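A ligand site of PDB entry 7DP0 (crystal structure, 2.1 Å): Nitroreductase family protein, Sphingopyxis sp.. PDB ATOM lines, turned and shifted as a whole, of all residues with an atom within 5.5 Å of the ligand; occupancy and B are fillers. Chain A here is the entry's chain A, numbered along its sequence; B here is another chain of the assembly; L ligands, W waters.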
ATOM      1  N   ARG A  18      -8.423 -10.396  12.652  1.00  0.00           N
ATOM      2  CA  ARG A  18      -7.969  -9.256  13.457  1.00  0.00           C
ATOM      3  C   ARG A  18      -7.157  -8.318  12.594  1.00  0.00           C
ATOM      4  O   ARG A  18      -6.206  -8.727  11.948  1.00  0.00           O
ATOM      5  CB  ARG A  18      -7.128  -9.684  14.675  1.00  0.00           C
ATOM      6  CG  ARG A  18      -6.784  -8.511  15.608  1.00  0.00           C
ATOM      7  CD  ARG A  18      -5.321  -8.503  16.097  1.00  0.00           C
ATOM      8  NE  ARG A  18      -4.388  -8.587  14.973  1.00  0.00           N
ATOM      9  CZ  ARG A  18      -3.976  -7.557  14.227  1.00  0.00           C
ATOM     10  NH1 ARG A  18      -4.384  -6.316  14.475  1.00  0.00           N
ATOM     11  NH2 ARG A  18      -3.144  -7.794  13.217  1.00  0.00           N
ATOM     12  N   ARG A  19      -7.551  -7.042  12.601  1.00  0.00           N
ATOM     13  CA  ARG A  19      -6.789  -5.981  11.946  1.00  0.00           C
ATOM     14  C   ARG A  19      -6.849  -4.756  12.815  1.00  0.00           C
ATOM     15  O   ARG A  19      -7.686  -4.665  13.724  1.00  0.00           O
ATOM     16  CB  ARG A  19      -7.364  -5.667  10.549  1.00  0.00           C
ATOM     17  CG  ARG A  19      -8.636  -4.844  10.569  1.00  0.00           C
ATOM     18  CD  ARG A  19      -9.109  -4.510   9.134  1.00  0.00           C
ATOM     19  NE  ARG A  19      -8.197  -3.597   8.459  1.00  0.00           N
ATOM     20  CZ  ARG A  19      -7.869  -3.653   7.161  1.00  0.00           C
ATOM     21  NH1 ARG A  19      -8.412  -4.568   6.376  1.00  0.00           N
ATOM     22  NH2 ARG A  19      -7.018  -2.776   6.644  1.00  0.00           N
ATOM     23  N   SER A  20      -5.963  -3.788  12.526  1.00  0.00           N
ATOM     24  CA  SER A  20      -5.998  -2.506  13.191  1.00  0.00           C
ATOM     25  C   SER A  20      -7.124  -1.626  12.607  1.00  0.00           C
ATOM     26  O   SER A  20      -6.991  -1.045  11.524  1.00  0.00           O
ATOM     27  CB  SER A  20      -4.639  -1.816  13.062  1.00  0.00           C
ATOM     28  OG  SER A  20      -3.687  -2.553  13.830  1.00  0.00           O
ATOM     29  N   ARG A  22      -9.446   1.493  12.107  1.00  0.00           N
ATOM     30  CA  ARG A  22      -9.298   2.929  12.272  1.00  0.00           C
ATOM     31  C   ARG A  22     -10.575   3.664  11.877  1.00  0.00           C
ATOM     32  O   ARG A  22     -10.532   4.816  11.446  1.00  0.00           O
ATOM     33  CB  ARG A  22      -8.093   3.416  11.460  1.00  0.00           C
ATOM     34  CG  ARG A  22      -6.801   2.749  11.920  1.00  0.00           C
ATOM     35  CD  ARG A  22      -5.652   3.096  11.021  1.00  0.00           C
ATOM     36  NE  ARG A  22      -4.420   2.485  11.495  1.00  0.00           N
ATOM     37  CZ  ARG A  22      -3.888   1.400  10.969  1.00  0.00           C
ATOM     38  NH1 ARG A  22      -4.507   0.799   9.953  1.00  0.00           N
ATOM     39  NH2 ARG A  22      -2.764   0.890  11.456  1.00  0.00           N
ATOM     40  N   VAL A 103       2.752  -0.292   4.593  1.00  0.00           N
ATOM     41  CA  VAL A 103       1.429  -0.302   5.209  1.00  0.00           C
ATOM     42  C   VAL A 103       0.807   1.106   5.171  1.00  0.00           C
ATOM     43  O   VAL A 103      -0.404   1.252   4.958  1.00  0.00           O
ATOM     44  CB  VAL A 103       1.463  -0.849   6.668  1.00  0.00           C
ATOM     45  CG1 VAL A 103       1.774   0.250   7.724  1.00  0.00           C
ATOM     46  CG2 VAL A 103       0.149  -1.513   6.992  1.00  0.00           C
ATOM     47  N   ASN A 128      -5.818   9.701  15.341  1.00  0.00           N
ATOM     48  CA  ASN A 128      -5.244   8.780  16.325  1.00  0.00           C
ATOM     49  C   ASN A 128      -5.606   9.185  17.744  1.00  0.00           C
ATOM     50  O   ASN A 128      -5.914   8.331  18.571  1.00  0.00           O
ATOM     51  CB  ASN A 128      -3.722   8.724  16.220  1.00  0.00           C
ATOM     52  CG  ASN A 128      -3.243   7.703  15.227  1.00  0.00           C
ATOM     53  OD1 ASN A 128      -3.146   6.520  15.540  1.00  0.00           O
ATOM     54  ND2 ASN A 128      -2.893   8.164  14.036  1.00  0.00           N
ATOM     55  N   PHE A 132      -9.691   7.171  16.878  1.00  0.00           N
ATOM     56  CA  PHE A 132     -10.444   6.842  15.663  1.00  0.00           C
ATOM     57  C   PHE A 132     -11.939   6.683  15.957  1.00  0.00           C
ATOM     58  O   PHE A 132     -12.631   5.900  15.296  1.00  0.00           O
ATOM     59  CB  PHE A 132      -9.897   5.573  14.993  1.00  0.00           C
ATOM     60  CG  PHE A 132      -8.463   5.686  14.550  1.00  0.00           C
ATOM     61  CD1 PHE A 132      -8.103   6.590  13.561  1.00  0.00           C
ATOM     62  CD2 PHE A 132      -7.474   4.883  15.114  1.00  0.00           C
ATOM     63  CE1 PHE A 132      -6.786   6.704  13.160  1.00  0.00           C
ATOM     64  CE2 PHE A 132      -6.146   4.986  14.700  1.00  0.00           C
ATOM     65  CZ  PHE A 132      -5.813   5.898  13.728  1.00  0.00           C
ATOM     66  N   LEU A 158      -1.636  -8.396  25.337  1.00  0.00           N
ATOM     67  CA  LEU A 158      -2.347  -7.504  24.416  1.00  0.00           C
ATOM     68  C   LEU A 158      -2.900  -8.277  23.198  1.00  0.00           C
ATOM     69  O   LEU A 158      -4.049  -8.078  22.814  1.00  0.00           O
ATOM     70  CB  LEU A 158      -1.435  -6.339  23.949  1.00  0.00           C
ATOM     71  CG  LEU A 158      -2.276  -5.211  23.340  1.00  0.00           C
ATOM     72  CD1 LEU A 158      -3.151  -4.563  24.443  1.00  0.00           C
ATOM     73  CD2 LEU A 158      -1.397  -4.168  22.686  1.00  0.00           C
ATOM     74  N   CYS A 173      -7.665  -1.087  17.785  1.00  0.00           N
ATOM     75  CA  CYS A 173      -6.466  -0.565  17.135  1.00  0.00           C
ATOM     76  C   CYS A 173      -5.443  -0.273  18.220  1.00  0.00           C
ATOM     77  O   CYS A 173      -5.680   0.567  19.069  1.00  0.00           O
ATOM     78  CB  CYS A 173      -6.758   0.694  16.337  1.00  0.00           C
ATOM     79  SG  CYS A 173      -5.276   1.361  15.471  1.00  0.00           S
ATOM     80  N   PRO A 174      -4.321  -0.998  18.214  1.00  0.00           N
ATOM     81  CA  PRO A 174      -3.241  -0.715  19.171  1.00  0.00           C
ATOM     82  C   PRO A 174      -2.552   0.588  18.793  1.00  0.00           C
ATOM     83  O   PRO A 174      -2.365   0.864  17.601  1.00  0.00           O
ATOM     84  CB  PRO A 174      -2.298  -1.928  19.014  1.00  0.00           C
ATOM     85  CG  PRO A 174      -2.656  -2.531  17.684  1.00  0.00           C
ATOM     86  CD  PRO A 174      -4.044  -2.174  17.360  1.00  0.00           C
ATOM     87  N   GLN A 175      -2.190   1.392  19.790  1.00  0.00           N
ATOM     88  CA  GLN A 175      -1.688   2.726  19.508  1.00  0.00           C
ATOM     89  C   GLN A 175      -0.500   3.127  20.384  1.00  0.00           C
ATOM     90  O   GLN A 175      -0.645   3.400  21.585  1.00  0.00           O
ATOM     91  CB  GLN A 175      -2.801   3.738  19.702  1.00  0.00           C
ATOM     92  CG  GLN A 175      -3.952   3.606  18.719  1.00  0.00           C
ATOM     93  CD  GLN A 175      -4.906   4.744  18.912  1.00  0.00           C
ATOM     94  OE1 GLN A 175      -5.643   4.782  19.914  1.00  0.00           O
ATOM     95  NE2 GLN A 175      -4.881   5.714  17.994  1.00  0.00           N
ATOM     96  N   GLU A 176       0.670   3.212  19.783  1.00  0.00           N
ATOM     97  CA  GLU A 176       1.838   3.693  20.492  1.00  0.00           C
ATOM     98  C   GLU A 176       1.927   5.225  20.430  1.00  0.00           C
ATOM     99  O   GLU A 176       2.779   5.829  21.088  1.00  0.00           O
ATOM    100  CB  GLU A 176       3.096   3.053  19.912  1.00  0.00           C
ATOM    101  CG  GLU A 176       3.429   1.766  20.600  1.00  0.00           C
ATOM    102  CD  GLU A 176       4.283   0.882  19.724  1.00  0.00           C
ATOM    103  OE1 GLU A 176       4.512   1.266  18.557  1.00  0.00           O
ATOM    104  OE2 GLU A 176       4.705  -0.208  20.193  1.00  0.00           O
ATOM    105  N   CYS A 177       1.076   5.842  19.626  1.00  0.00           N
ATOM    106  CA  CYS A 177       1.091   7.300  19.503  1.00  0.00           C
ATOM    107  C   CYS A 177       0.837   7.976  20.872  1.00  0.00           C
ATOM    108  O   CYS A 177       1.325   9.084  21.131  1.00  0.00           O
ATOM    109  CB  CYS A 177       0.056   7.776  18.468  1.00  0.00           C
ATOM    110  SG  CYS A 177      -1.632   7.330  18.908  1.00  0.00           S
ATOM    111  N   TRP A 178       0.107   7.285  21.744  1.00  0.00           N
ATOM    112  CA  TRP A 178      -0.117   7.805  23.109  1.00  0.00           C
ATOM    113  C   TRP A 178       1.180   7.953  23.925  1.00  0.00           C
ATOM    114  O   TRP A 178       1.278   8.846  24.791  1.00  0.00           O
ATOM    115  CB  TRP A 178      -1.119   6.898  23.842  1.00  0.00           C
ATOM    116  CG  TRP A 178      -2.428   6.942  23.166  1.00  0.00           C
ATOM    117  CD1 TRP A 178      -2.933   6.027  22.307  1.00  0.00           C
ATOM    118  CD2 TRP A 178      -3.387   8.003  23.250  1.00  0.00           C
ATOM    119  NE1 TRP A 178      -4.162   6.444  21.853  1.00  0.00           N
ATOM    120  CE2 TRP A 178      -4.463   7.640  22.417  1.00  0.00           C
ATOM    121  CE3 TRP A 178      -3.447   9.215  23.949  1.00  0.00           C
ATOM    122  CZ2 TRP A 178      -5.602   8.468  22.255  1.00  0.00           C
ATOM    123  CZ3 TRP A 178      -4.569  10.028  23.797  1.00  0.00           C
ATOM    124  CH2 TRP A 178      -5.642   9.638  22.958  1.00  0.00           C
ATOM    125  N   PHE A 198       3.065   1.956  28.008  1.00  0.00           N
ATOM    126  CA  PHE A 198       3.515   1.298  26.782  1.00  0.00           C
ATOM    127  C   PHE A 198       2.639   1.699  25.602  1.00  0.00           C
ATOM    128  O   PHE A 198       3.115   2.312  24.663  1.00  0.00           O
ATOM    129  CB  PHE A 198       3.534  -0.240  26.949  1.00  0.00           C
ATOM    130  CG  PHE A 198       3.545  -1.005  25.635  1.00  0.00           C
ATOM    131  CD1 PHE A 198       4.317  -0.575  24.551  1.00  0.00           C
ATOM    132  CD2 PHE A 198       2.788  -2.158  25.482  1.00  0.00           C
ATOM    133  CE1 PHE A 198       4.318  -1.278  23.346  1.00  0.00           C
ATOM    134  CE2 PHE A 198       2.790  -2.875  24.274  1.00  0.00           C
ATOM    135  CZ  PHE A 198       3.537  -2.433  23.220  1.00  0.00           C
ATOM    136  N   SER A 199       1.364   1.362  25.656  1.00  0.00           N
ATOM    137  CA  SER A 199       0.518   1.508  24.491  1.00  0.00           C
ATOM    138  C   SER A 199      -0.935   1.742  24.871  1.00  0.00           C
ATOM    139  O   SER A 199      -1.346   1.403  25.977  1.00  0.00           O
ATOM    140  CB  SER A 199       0.615   0.261  23.608  1.00  0.00           C
ATOM    141  OG  SER A 199      -0.146   0.406  22.421  1.00  0.00           O
ATOM    142  N   TRP A 215      -8.887  -2.426   3.271  1.00  0.00           N
ATOM    143  CA  TRP A 215      -7.741  -2.694   2.417  1.00  0.00           C
ATOM    144  C   TRP A 215      -6.935  -3.865   2.971  1.00  0.00           C
ATOM    145  O   TRP A 215      -6.808  -4.017   4.182  1.00  0.00           O
ATOM    146  CB  TRP A 215      -6.878  -1.441   2.307  1.00  0.00           C
ATOM    147  CG  TRP A 215      -6.551  -0.856   3.641  1.00  0.00           C
ATOM    148  CD1 TRP A 215      -7.387  -0.115   4.419  1.00  0.00           C
ATOM    149  CD2 TRP A 215      -5.324  -0.976   4.356  1.00  0.00           C
ATOM    150  NE1 TRP A 215      -6.755   0.239   5.592  1.00  0.00           N
ATOM    151  CE2 TRP A 215      -5.475  -0.279   5.580  1.00  0.00           C
ATOM    152  CE3 TRP A 215      -4.109  -1.613   4.101  1.00  0.00           C
ATOM    153  CZ2 TRP A 215      -4.466  -0.199   6.536  1.00  0.00           C
ATOM    154  CZ3 TRP A 215      -3.095  -1.525   5.052  1.00  0.00           C
ATOM    155  CH2 TRP A 215      -3.277  -0.825   6.250  1.00  0.00           C
ATOM    156  N   VAL A 217      -3.955  -5.788   4.323  1.00  0.00           N
ATOM    157  CA  VAL A 217      -2.710  -5.393   4.995  1.00  0.00           C
ATOM    158  C   VAL A 217      -1.606  -6.424   4.718  1.00  0.00           C
ATOM    159  O   VAL A 217      -1.803  -7.618   4.909  1.00  0.00           O
ATOM    160  CB  VAL A 217      -2.914  -5.238   6.496  1.00  0.00           C
ATOM    161  CG1 VAL A 217      -1.682  -4.586   7.151  1.00  0.00           C
ATOM    162  CG2 VAL A 217      -4.185  -4.437   6.773  1.00  0.00           C
ATOM    163  N   ARG A 219       2.155  -8.535   4.726  1.00  0.00           N
ATOM    164  CA  ARG A 219       3.111  -9.148   5.655  1.00  0.00           C
ATOM    165  C   ARG A 219       4.242  -9.702   4.802  1.00  0.00           C
ATOM    166  O   ARG A 219       3.997 -10.147   3.694  1.00  0.00           O
ATOM    167  CB  ARG A 219       2.476 -10.291   6.476  1.00  0.00           C
ATOM    168  CG  ARG A 219       1.498  -9.883   7.595  1.00  0.00           C
ATOM    169  CD  ARG A 219       2.094  -8.943   8.612  1.00  0.00           C
ATOM    170  NE  ARG A 219       1.158  -8.783   9.719  1.00  0.00           N
ATOM    171  CZ  ARG A 219       0.103  -7.962   9.688  1.00  0.00           C
ATOM    172  NH1 ARG A 219      -0.107  -7.213   8.605  1.00  0.00           N
ATOM    173  NH2 ARG A 219      -0.723  -7.883  10.721  1.00  0.00           N
ATOM    174  N   ARG B  43       0.318 -12.917  10.810  1.00  0.00           N
ATOM    175  CA  ARG B  43      -0.755 -11.917  10.850  1.00  0.00           C
ATOM    176  C   ARG B  43      -0.841 -11.180  12.186  1.00  0.00           C
ATOM    177  O   ARG B  43      -1.665 -10.267  12.373  1.00  0.00           O
ATOM    178  CB  ARG B  43      -2.105 -12.581  10.575  1.00  0.00           C
ATOM    179  CG  ARG B  43      -2.185 -13.305   9.232  1.00  0.00           C
ATOM    180  CD  ARG B  43      -1.821 -12.405   8.039  1.00  0.00           C
ATOM    181  NE  ARG B  43      -2.523 -11.122   8.065  1.00  0.00           N
ATOM    182  CZ  ARG B  43      -2.446 -10.209   7.097  1.00  0.00           C
ATOM    183  NH1 ARG B  43      -1.736 -10.439   5.999  1.00  0.00           N
ATOM    184  NH2 ARG B  43      -3.107  -9.059   7.214  1.00  0.00           N
ATOM    185  N   ALA B  44       0.026 -11.562  13.118  1.00  0.00           N
ATOM    186  CA  ALA B  44       0.155 -10.832  14.360  1.00  0.00           C
ATOM    187  C   ALA B  44       0.441  -9.339  14.052  1.00  0.00           C
ATOM    188  O   ALA B  44       1.085  -9.020  13.042  1.00  0.00           O
ATOM    189  CB  ALA B  44       1.243 -11.442  15.213  1.00  0.00           C
ATOM    190  N   PRO B  45      -0.072  -8.421  14.874  1.00  0.00           N
ATOM    191  CA  PRO B  45       0.261  -7.014  14.580  1.00  0.00           C
ATOM    192  C   PRO B  45       1.650  -6.643  15.071  1.00  0.00           C
ATOM    193  O   PRO B  45       2.270  -7.389  15.821  1.00  0.00           O
ATOM    194  CB  PRO B  45      -0.825  -6.224  15.345  1.00  0.00           C
ATOM    195  CG  PRO B  45      -1.120  -7.109  16.536  1.00  0.00           C
ATOM    196  CD  PRO B  45      -0.978  -8.552  16.022  1.00  0.00           C
ATOM    197  N   SER B  46       2.129  -5.475  14.675  1.00  0.00           N
ATOM    198  CA  SER B  46       3.359  -4.959  15.256  1.00  0.00           C
ATOM    199  C   SER B  46       3.393  -3.442  15.041  1.00  0.00           C
ATOM    200  O   SER B  46       2.789  -2.926  14.095  1.00  0.00           O
ATOM    201  CB  SER B  46       4.596  -5.660  14.647  1.00  0.00           C
ATOM    202  OG  SER B  46       4.678  -5.507  13.243  1.00  0.00           O
ATOM    203  N   GLY B  47       4.032  -2.729  15.955  1.00  0.00           N
ATOM    204  CA  GLY B  47       4.180  -1.285  15.800  1.00  0.00           C
ATOM    205  C   GLY B  47       4.770  -0.958  14.441  1.00  0.00           C
ATOM    206  O   GLY B  47       5.802  -1.501  14.100  1.00  0.00           O
ATOM    207  N   GLY B  48       4.082  -0.156  13.638  1.00  0.00           N
ATOM    208  CA  GLY B  48       4.547   0.203  12.303  1.00  0.00           C
ATOM    209  C   GLY B  48       4.677  -0.969  11.328  1.00  0.00           C
ATOM    210  O   GLY B  48       5.384  -0.868  10.314  1.00  0.00           O
ATOM    211  N   ASN B  49       4.012  -2.083  11.622  1.00  0.00           N
ATOM    212  CA  ASN B  49       4.136  -3.304  10.832  1.00  0.00           C
ATOM    213  C   ASN B  49       5.615  -3.707  10.664  1.00  0.00           C
ATOM    214  O   ASN B  49       6.013  -4.297   9.658  1.00  0.00           O
ATOM    215  CB  ASN B  49       3.472  -3.133   9.446  1.00  0.00           C
ATOM    216  CG  ASN B  49       3.087  -4.466   8.816  1.00  0.00           C
ATOM    217  OD1 ASN B  49       2.709  -5.420   9.500  1.00  0.00           O
ATOM    218  ND2 ASN B  49       3.144  -4.521   7.479  1.00  0.00           N
ATOM    219  N   PRO B 149       9.377  -1.739  22.757  1.00  0.00           N
ATOM    220  CA  PRO B 149       8.079  -1.943  22.089  1.00  0.00           C
ATOM    221  C   PRO B 149       8.181  -3.041  21.033  1.00  0.00           C
ATOM    222  O   PRO B 149       7.200  -3.766  20.815  1.00  0.00           O
ATOM    223  CB  PRO B 149       7.790  -0.579  21.436  1.00  0.00           C
ATOM    224  CG  PRO B 149       9.173   0.012  21.209  1.00  0.00           C
ATOM    225  CD  PRO B 149       9.963  -0.424  22.407  1.00  0.00           C
ATOM    226  N   ASP B 153       6.195  -6.589  20.419  1.00  0.00           N
ATOM    227  CA  ASP B 153       5.784  -7.155  19.122  1.00  0.00           C
ATOM    228  C   ASP B 153       6.072  -8.659  19.044  1.00  0.00           C
ATOM    229  O   ASP B 153       5.247  -9.447  18.565  1.00  0.00           O
ATOM    230  CB  ASP B 153       6.518  -6.484  17.954  1.00  0.00           C
ATOM    231  CG  ASP B 153       6.249  -5.000  17.809  1.00  0.00           C
ATOM    232  OD1 ASP B 153       5.229  -4.469  18.303  1.00  0.00           O
ATOM    233  OD2 ASP B 153       7.123  -4.356  17.179  1.00  0.00           O
ATOM    234  N   MET B 156       3.554 -10.601  20.935  1.00  0.00           N
ATOM    235  CA  MET B 156       2.307 -10.777  20.165  1.00  0.00           C
ATOM    236  C   MET B 156       2.435 -11.954  19.177  1.00  0.00           C
ATOM    237  O   MET B 156       1.488 -12.723  18.976  1.00  0.00           O
ATOM    238  CB  MET B 156       1.982  -9.506  19.391  1.00  0.00           C
ATOM    239  CG  MET B 156       1.759  -8.280  20.310  1.00  0.00           C
ATOM    240  SD  MET B 156       1.753  -6.685  19.478  1.00  0.00           S
ATOM    241  CE  MET B 156       1.997  -5.590  20.931  1.00  0.00           C
HETATM  242  N1  LIG L   1      -1.633   2.098  14.146  1.00  0.00           N
HETATM  243  C1  LIG L   1      -1.874   3.470  14.156  1.00  0.00           C
HETATM  244  O1  LIG L   1      -2.503   4.015  13.256  1.00  0.00           O
HETATM  245  N2  LIG L   1      -1.437   4.283  15.174  1.00  0.00           N
HETATM  246  C2  LIG L   1      -0.733   3.763  16.219  1.00  0.00           C
HETATM  247  O2  LIG L   1      -0.374   4.512  17.136  1.00  0.00           O
HETATM  248  C3  LIG L   1      -0.461   2.393  16.219  1.00  0.00           C
HETATM  249  N3  LIG L   1       0.242   1.869  17.280  1.00  0.00           N
HETATM  250  C4  LIG L   1       0.509   0.518  17.350  1.00  0.00           C
HETATM  251  C5  LIG L   1       1.216   0.040  18.440  1.00  0.00           C
HETATM  252  C6  LIG L   1       1.495  -1.303  18.543  1.00  0.00           C
HETATM  253  C7  LIG L   1       2.247  -1.857  19.727  1.00  0.00           C
HETATM  254  C8  LIG L   1       1.079  -2.172  17.555  1.00  0.00           C
HETATM  255  C9  LIG L   1       1.397  -3.617  17.709  1.00  0.00           C
HETATM  256  C10 LIG L   1       0.381  -1.690  16.454  1.00  0.00           C
HETATM  257  C11 LIG L   1       0.078  -0.332  16.335  1.00  0.00           C
HETATM  258  N4  LIG L   1      -0.628   0.183  15.247  1.00  0.00           N
HETATM  259  C12 LIG L   1      -0.911   1.549  15.198  1.00  0.00           C
HETATM  260  C13 LIG L   1      -1.119  -0.730  14.158  1.00  0.00           C
HETATM  261  C14 LIG L   1      -0.016  -1.140  13.170  1.00  0.00           C
HETATM  262  O3  LIG L   1       0.238  -0.128  12.237  1.00  0.00           O
HETATM  263  C15 LIG L   1      -0.494  -2.420  12.484  1.00  0.00           C
HETATM  264  O4  LIG L   1      -0.551  -3.410  13.483  1.00  0.00           O
HETATM  265  C16 LIG L   1       0.360  -2.945  11.312  1.00  0.00           C
HETATM  266  O5  LIG L   1       0.291  -2.091  10.184  1.00  0.00           O
HETATM  267  C17 LIG L   1      -0.215  -4.290  10.899  1.00  0.00           C
HETATM  268  O6  LIG L   1      -1.522  -4.059  10.363  1.00  0.00           O
HETATM  269  P1  LIG L   1      -2.821  -4.764  11.001  1.00  0.00           P
HETATM  270  O7  LIG L   1      -4.046  -3.968  10.584  1.00  0.00           O
HETATM  271  O8  LIG L   1      -2.762  -4.799  12.501  1.00  0.00           O
HETATM  272  O9  LIG L   1      -2.889  -6.189  10.470  1.00  0.00           O
HETATM  273  O   HOH W   1      -2.066  -1.468   9.582  1.00  0.00           O
HETATM  274  O   HOH W   2       1.851   2.022  13.376  1.00  0.00           O
HETATM  275  O   HOH W   3      -2.207   6.144  11.693  1.00  0.00           O
HETATM  276  O   HOH W   4      -4.654  -7.810   9.502  1.00  0.00           O
HETATM  277  O   HOH W   5      -5.614  -2.427   9.265  1.00  0.00           O
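The backbone NH (N) of Ser 20 lies within hydrogen-bond range of an oxygen (O7) of the ligand, at 2.7 Å. O8 of the ligand lies within hydrogen-bond range of OG of Ser 20. An oxygen (O9) of the ligand is in salt-bridge range of the guanidinium group of Arg 219, 2.8 Å away. The side-chain amide oxygen of Asn 128 is in hydrogen-bond range of a nitrogen (N2) of the ligand, 2.8 Å away. N of Glu 176 sits at hydrogen-bond distance from N3 of the ligand (2.9 Å). O8 of the ligand lies within salt-bridge range of NH1 of Arg 18, at 3.0 Å. The guanidinium group (NE) of Arg 22 sits at hydrogen-bond distance from an oxygen (O1) of the ligand. O2 of the ligand lies within hydrogen-bond range of N of Cys 177 (3.2 Å). An oxygen (O2) of the ligand lies close to the side-chain sulfur (SG) of Cys 177 (3.6 Å). An oxygen (O4) of the ligand is in hydrogen-bond range of the backbone carbonyl oxygen (O) of Ser 46 of chain B (3.4 Å).
The guanidinium group (NH1) of Arg 219 sits at hydrogen-bond distance from the side-chain amide oxygen (OD1) of Asn 49 of chain B (3.5 Å). NH2 of Arg 219 sits at hydrogen-bond distance from O of Arg 43 of chain B. The guanidinium group (NH2) of Arg 219 lies within hydrogen-bond range of the backbone carbonyl oxygen (O) of Ala 44 of chain B, at 3.2 Å. NE2 of Gln 175 lies within hydrogen-bond range of SG of Cys 177, 3.7 Å away. The backbone carbonyl oxygen (O) of Gln 175 sits at hydrogen-bond distance from the side-chain hydroxyl (OG) of Ser 199 (3.1 Å). OE1 of Gln 175 lies within hydrogen-bond range of NE1 of Trp 178 (3.0 Å). The backbone carbonyl oxygen (O) of Val 217 sits at hydrogen-bond distance from the guanidinium group (NH2) of Arg 43 of chain B (3.0 Å). O of Trp 215 sits at hydrogen-bond distance from NH2 of Arg 19 (2.8 Å).
The backbone carbonyl oxygen (O) of Pro 174 sits close to a nitrogen (N3) of the ligand, 2.8 Å away. Residues that only touch the ligand: Gln 175 (3.1 Å), Val 103 (3.2 Å), Val 217 (3.3 Å), Gly 47 of chain B (3.3 Å), Pro 45 of chain B (3.4 Å), Asn 49 of chain B (3.4 Å), Met 156 of chain B (3.6 Å), Arg 19 (3.7 Å), Phe 198 (3.8 Å), Phe 132 (3.8 Å), Cys 173 (3.9 Å) and Asp 153 of chain B (3.97 Å). Hydrophobic or aromatic side chains within 4 Å of the ligand: Val 103, Phe 132, Pro 174, Phe 198, Val 217, Pro 45 of chain B and Met 156 of chain B. Along chain A the residues within 4 Å of the ligand span positions 18 to 219. The nearest printed residue that does not touch the ligand is Gly 48 of chain B (4.1 Å).
Water W1 bridges an oxygen (O5) of the ligand (2.5 Å) and the guanidinium group (NH2) of Arg 22 (3.1 Å). Water W5 lies within hydrogen-bond range of O7 of the ligand (2.6 Å), NE of Arg 19 (2.9 Å), O of Ser 20 (3.0 Å) and NH1 of Arg 22 (3.5 Å). Water W4 lies within hydrogen-bond range of O9 of the ligand (2.6 Å), NH2 of Arg 43 of chain B (3.0 Å) and O of Arg 18 (3.0 Å). Water W3 bridges O1 of the ligand and ND2 of Asn 128. Water W2 bridges O3 of the ligand (2.9 Å) and N of Gly 48 of chain B (3.1 Å).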
